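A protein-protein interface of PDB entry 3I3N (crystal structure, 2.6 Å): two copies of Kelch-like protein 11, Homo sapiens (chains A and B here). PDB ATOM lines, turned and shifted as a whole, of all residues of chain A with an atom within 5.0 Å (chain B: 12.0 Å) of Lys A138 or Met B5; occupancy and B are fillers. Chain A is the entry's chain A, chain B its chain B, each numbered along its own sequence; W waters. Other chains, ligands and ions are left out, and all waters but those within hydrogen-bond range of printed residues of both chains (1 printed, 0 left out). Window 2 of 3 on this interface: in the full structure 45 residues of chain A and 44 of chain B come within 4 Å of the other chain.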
ATOM      1  N   THR A 109       0.943   8.056  22.098  1.00  0.00           N
ATOM      2  CA  THR A 109       0.793   7.338  20.830  1.00  0.00           C
ATOM      3  C   THR A 109       1.455   8.088  19.691  1.00  0.00           C
ATOM      4  O   THR A 109       1.902   7.489  18.697  1.00  0.00           O
ATOM      5  CB  THR A 109      -0.705   7.146  20.482  1.00  0.00           C
ATOM      6  OG1 THR A 109      -1.518   7.765  21.498  1.00  0.00           O
ATOM      7  CG2 THR A 109      -1.053   5.649  20.386  1.00  0.00           C
ATOM      8  N   PHE A 134       3.866  -0.215  26.596  1.00  0.00           N
ATOM      9  CA  PHE A 134       2.927   0.783  26.142  1.00  0.00           C
ATOM     10  C   PHE A 134       2.274   0.296  24.859  1.00  0.00           C
ATOM     11  O   PHE A 134       1.044   0.254  24.747  1.00  0.00           O
ATOM     12  CB  PHE A 134       3.651   2.085  25.882  1.00  0.00           C
ATOM     13  CG  PHE A 134       2.769   3.158  25.351  1.00  0.00           C
ATOM     14  CD1 PHE A 134       2.019   3.951  26.211  1.00  0.00           C
ATOM     15  CD2 PHE A 134       2.697   3.389  23.985  1.00  0.00           C
ATOM     16  CE1 PHE A 134       1.211   4.961  25.718  1.00  0.00           C
ATOM     17  CE2 PHE A 134       1.888   4.398  23.484  1.00  0.00           C
ATOM     18  CZ  PHE A 134       1.146   5.185  24.354  1.00  0.00           C
ATOM     19  N   LEU A 135       3.111  -0.074  23.893  1.00  0.00           N
ATOM     20  CA  LEU A 135       2.637  -0.562  22.599  1.00  0.00           C
ATOM     21  C   LEU A 135       1.847  -1.854  22.736  1.00  0.00           C
ATOM     22  O   LEU A 135       0.841  -2.052  22.061  1.00  0.00           O
ATOM     23  CB  LEU A 135       3.816  -0.786  21.657  1.00  0.00           C
ATOM     24  CG  LEU A 135       4.521   0.493  21.210  1.00  0.00           C
ATOM     25  CD1 LEU A 135       5.771   0.156  20.436  1.00  0.00           C
ATOM     26  CD2 LEU A 135       3.571   1.325  20.361  1.00  0.00           C
ATOM     27  N   LYS A 136       2.308  -2.721  23.624  1.00  0.00           N
ATOM     28  CA  LYS A 136       1.674  -4.004  23.863  1.00  0.00           C
ATOM     29  C   LYS A 136       0.223  -3.852  24.343  1.00  0.00           C
ATOM     30  O   LYS A 136      -0.631  -4.690  24.051  1.00  0.00           O
ATOM     31  CB  LYS A 136       2.525  -4.771  24.883  1.00  0.00           C
ATOM     32  CG  LYS A 136       2.117  -6.212  25.143  1.00  0.00           C
ATOM     33  CD  LYS A 136       3.353  -7.104  25.321  1.00  0.00           C
ATOM     34  CE  LYS A 136       4.312  -6.558  26.381  1.00  0.00           C
ATOM     35  NZ  LYS A 136       5.562  -7.366  26.523  1.00  0.00           N
ATOM     36  N   LYS A 137      -0.055  -2.771  25.065  1.00  0.00           N
ATOM     37  CA  LYS A 137      -1.392  -2.509  25.590  1.00  0.00           C
ATOM     38  C   LYS A 137      -2.253  -1.764  24.580  1.00  0.00           C
ATOM     39  O   LYS A 137      -3.472  -1.731  24.705  1.00  0.00           O
ATOM     40  CB  LYS A 137      -1.298  -1.687  26.879  1.00  0.00           C
ATOM     41  CG  LYS A 137      -0.727  -2.450  28.062  1.00  0.00           C
ATOM     42  CD  LYS A 137      -0.058  -1.524  29.094  1.00  0.00           C
ATOM     43  CE  LYS A 137      -1.022  -0.525  29.724  1.00  0.00           C
ATOM     44  NZ  LYS A 137      -0.347   0.280  30.788  1.00  0.00           N
ATOM     45  N   LYS A 138      -1.614  -1.168  23.583  1.00  0.00           N
ATOM     46  CA  LYS A 138      -2.321  -0.418  22.556  1.00  0.00           C
ATOM     47  C   LYS A 138      -2.487  -1.243  21.280  1.00  0.00           C
ATOM     48  O   LYS A 138      -3.125  -0.801  20.319  1.00  0.00           O
ATOM     49  CB  LYS A 138      -1.564   0.881  22.258  1.00  0.00           C
ATOM     50  CG  LYS A 138      -1.895   2.019  23.201  1.00  0.00           C
ATOM     51  CD  LYS A 138      -3.315   2.469  22.936  1.00  0.00           C
ATOM     52  CE  LYS A 138      -3.692   3.713  23.714  1.00  0.00           C
ATOM     53  NZ  LYS A 138      -5.041   4.208  23.314  1.00  0.00           N
ATOM     54  N   LEU A 139      -1.919  -2.446  21.284  1.00  0.00           N
ATOM     55  CA  LEU A 139      -1.979  -3.337  20.129  1.00  0.00           C
ATOM     56  C   LEU A 139      -3.412  -3.484  19.643  1.00  0.00           C
ATOM     57  O   LEU A 139      -4.305  -3.824  20.414  1.00  0.00           O
ATOM     58  CB  LEU A 139      -1.431  -4.715  20.485  1.00  0.00           C
ATOM     59  CG  LEU A 139      -0.466  -5.351  19.487  1.00  0.00           C
ATOM     60  CD1 LEU A 139      -0.351  -6.813  19.823  1.00  0.00           C
ATOM     61  CD2 LEU A 139      -0.948  -5.179  18.067  1.00  0.00           C
ATOM     62  N   HIS A 140      -3.623  -3.242  18.354  1.00  0.00           N
ATOM     63  CA  HIS A 140      -4.958  -3.325  17.784  1.00  0.00           C
ATOM     64  C   HIS A 140      -4.930  -3.598  16.270  1.00  0.00           C
ATOM     65  O   HIS A 140      -4.065  -3.104  15.544  1.00  0.00           O
ATOM     66  CB  HIS A 140      -5.699  -2.025  18.119  1.00  0.00           C
ATOM     67  CG  HIS A 140      -7.051  -1.899  17.490  1.00  0.00           C
ATOM     68  ND1 HIS A 140      -7.243  -1.339  16.244  1.00  0.00           N
ATOM     69  CD2 HIS A 140      -8.282  -2.218  17.955  1.00  0.00           C
ATOM     70  CE1 HIS A 140      -8.536  -1.316  15.970  1.00  0.00           C
ATOM     71  NE2 HIS A 140      -9.189  -1.843  16.991  1.00  0.00           N
ATOM     72  N   ASN A 143      -3.359  -1.307  13.846  1.00  0.00           N
ATOM     73  CA  ASN A 143      -1.960  -0.883  13.896  1.00  0.00           C
ATOM     74  C   ASN A 143      -0.989  -2.032  14.088  1.00  0.00           C
ATOM     75  O   ASN A 143       0.212  -1.813  14.167  1.00  0.00           O
ATOM     76  CB  ASN A 143      -1.735   0.123  15.030  1.00  0.00           C
ATOM     77  CG  ASN A 143      -2.113  -0.442  16.399  1.00  0.00           C
ATOM     78  OD1 ASN A 143      -1.916  -1.634  16.677  1.00  0.00           O
ATOM     79  ND2 ASN A 143      -2.647   0.415  17.265  1.00  0.00           N
ATOM     80  N   ILE A 147       3.027  -1.736  14.102  1.00  0.00           N
ATOM     81  CA  ILE A 147       3.634  -2.120  15.359  1.00  0.00           C
ATOM     82  C   ILE A 147       4.561  -3.321  15.200  1.00  0.00           C
ATOM     83  O   ILE A 147       5.671  -3.320  15.726  1.00  0.00           O
ATOM     84  CB  ILE A 147       2.545  -2.399  16.442  1.00  0.00           C
ATOM     85  CG1 ILE A 147       1.898  -1.072  16.855  1.00  0.00           C
ATOM     86  CG2 ILE A 147       3.154  -3.108  17.653  1.00  0.00           C
ATOM     87  CD1 ILE A 147       0.891  -1.172  17.982  1.00  0.00           C
ATOM     88  N   SER B   4      -8.651   5.797  22.602  1.00  0.00           N
ATOM     89  CA  SER B   4      -7.444   5.299  21.880  1.00  0.00           C
ATOM     90  C   SER B   4      -6.282   6.303  21.975  1.00  0.00           C
ATOM     91  O   SER B   4      -5.151   6.017  21.559  1.00  0.00           O
ATOM     92  CB  SER B   4      -7.793   4.998  20.412  1.00  0.00           C
ATOM     93  OG  SER B   4      -8.524   6.060  19.821  1.00  0.00           O
ATOM     94  N   MET B   5      -6.572   7.481  22.522  1.00  0.00           N
ATOM     95  CA  MET B   5      -5.555   8.511  22.715  1.00  0.00           C
ATOM     96  C   MET B   5      -5.093   8.348  24.152  1.00  0.00           C
ATOM     97  O   MET B   5      -5.904   8.141  25.061  1.00  0.00           O
ATOM     98  CB  MET B   5      -6.136   9.917  22.541  1.00  0.00           C
ATOM     99  CG  MET B   5      -5.491  10.720  21.428  1.00  0.00           C
ATOM    100  SD  MET B   5      -5.810  12.617  21.607  1.00  0.00           S
ATOM    101  CE  MET B   5      -4.137  13.067  22.426  1.00  0.00           C
ATOM    102  N   GLU B   6      -3.796   8.448  24.372  1.00  0.00           N
ATOM    103  CA  GLU B   6      -3.310   8.276  25.718  1.00  0.00           C
ATOM    104  C   GLU B   6      -1.845   8.634  25.823  1.00  0.00           C
ATOM    105  O   GLU B   6      -1.089   8.598  24.856  1.00  0.00           O
ATOM    106  CB  GLU B   6      -3.560   6.826  26.158  1.00  0.00           C
ATOM    107  CG  GLU B   6      -2.793   6.364  27.392  1.00  0.00           C
ATOM    108  CD  GLU B   6      -3.045   4.894  27.756  1.00  0.00           C
ATOM    109  OE1 GLU B   6      -3.084   4.031  26.839  1.00  0.00           O
ATOM    110  OE2 GLU B   6      -3.183   4.600  28.968  1.00  0.00           O
ATOM    111  N   ALA B   7      -1.455   9.020  27.015  1.00  0.00           N
ATOM    112  CA  ALA B   7      -0.087   9.369  27.279  1.00  0.00           C
ATOM    113  C   ALA B   7       0.108   8.794  28.660  1.00  0.00           C
ATOM    114  O   ALA B   7      -0.743   8.973  29.530  1.00  0.00           O
ATOM    115  CB  ALA B   7       0.082  10.862  27.293  1.00  0.00           C
ATOM    116  N   GLU B   8       1.201   8.073  28.854  1.00  0.00           N
ATOM    117  CA  GLU B   8       1.455   7.488  30.154  1.00  0.00           C
ATOM    118  C   GLU B   8       2.803   7.967  30.679  1.00  0.00           C
ATOM    119  O   GLU B   8       3.777   8.055  29.933  1.00  0.00           O
ATOM    120  CB  GLU B   8       1.434   5.967  30.038  1.00  0.00           C
ATOM    121  CG  GLU B   8       1.340   5.256  31.367  1.00  0.00           C
ATOM    122  CD  GLU B   8       1.414   3.749  31.218  1.00  0.00           C
ATOM    123  OE1 GLU B   8       1.517   3.059  32.260  1.00  0.00           O
ATOM    124  OE2 GLU B   8       1.367   3.257  30.063  1.00  0.00           O
ATOM    125  N   ASP B   9       2.845   8.310  31.958  1.00  0.00           N
ATOM    126  CA  ASP B   9       4.077   8.761  32.586  1.00  0.00           C
ATOM    127  C   ASP B   9       4.870   7.551  33.065  1.00  0.00           C
ATOM    128  O   ASP B   9       4.319   6.666  33.720  1.00  0.00           O
ATOM    129  CB  ASP B   9       3.776   9.655  33.792  1.00  0.00           C
ATOM    130  CG  ASP B   9       3.299  11.039  33.393  1.00  0.00           C
ATOM    131  OD1 ASP B   9       3.090  11.884  34.292  1.00  0.00           O
ATOM    132  OD2 ASP B   9       3.137  11.281  32.181  1.00  0.00           O
HETATM  133  O   HOH W   1       1.967   0.667  29.860  1.00  0.00           O
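No position is printed for both chains. Of the 6 pairs that touch across the chains among the printed residues, none has its exchanged pair printed and touching as well.
Phe A134 touches Glu B8 (CD1 to OE2, 3.97 Å). Lys A138 touches Met B5 (NZ to N, 3.7 Å). Lys A138 touches Glu B6.
Lys A138 touches just these residues of chain B: Ser B4, Met B5 and Glu B6. Met B5 touches just one residue of chain A: Lys A138 (3.7 Å). Leu A135 touches none of the printed residues of chain B. Of chain B, only Glu B8 (3.5 Å) comes within 4 Å of Lys A137. No residue of chain B comes within 4 Å of Leu A139. His A140 touches none of the printed residues of chain B. No residue of chain B comes within 4 Å of Asn A143. Of the printed residues of chain B, Thr A109 touches Glu B6 (3.5 Å). Of the printed residues of chain A, Ser B4 touches Lys A138. Lys A136 touches none of the printed residues of chain B. Asp B9 touches none of the printed residues of chain A. The nearest residue of chain B that does not touch Lys A138 is Ala B7 (6.6 Å). The nearest residue of chain A that does not touch Met B5 is Thr A109 (4.3 Å). The nearest printed residue of chain A that does not touch Glu B8 is Thr A109 (6.8 Å).
Of the 10 printed residues of chain A, 4 touch a printed residue of chain B. Hydrophobic or aromatic side chains of chain A within 4 Å of the printed part of chain B: Phe A134. Among the printed residues, 6 pairs touch across the chains. Among the printed residues, Asp or Glu carboxylates within 4 Å of a Lys or Arg side-chain nitrogen of the other chain: Lys A137 with Glu B8 (3.5 Å).
N of Thr A109 sits at hydrogen-bond distance from O of Glu B6, 3.5 Å away. The side-chain amino group of Lys A137 lies within salt-bridge range of the side-chain carboxylate of Glu B8 (3.5 Å). The side-chain amino group (NZ) of Lys A138 is in hydrogen-bond range of the backbone carbonyl oxygen (O) of Ser B4.
Water W1 lies within hydrogen-bond range of the side-chain amino group of Lys A137 (2.5 Å) and the side-chain carboxylate of Glu B8 (2.7 Å).
ND2 of Asn A143 is in hydrogen-bond range of O of Lys A138 (3.3 Å).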
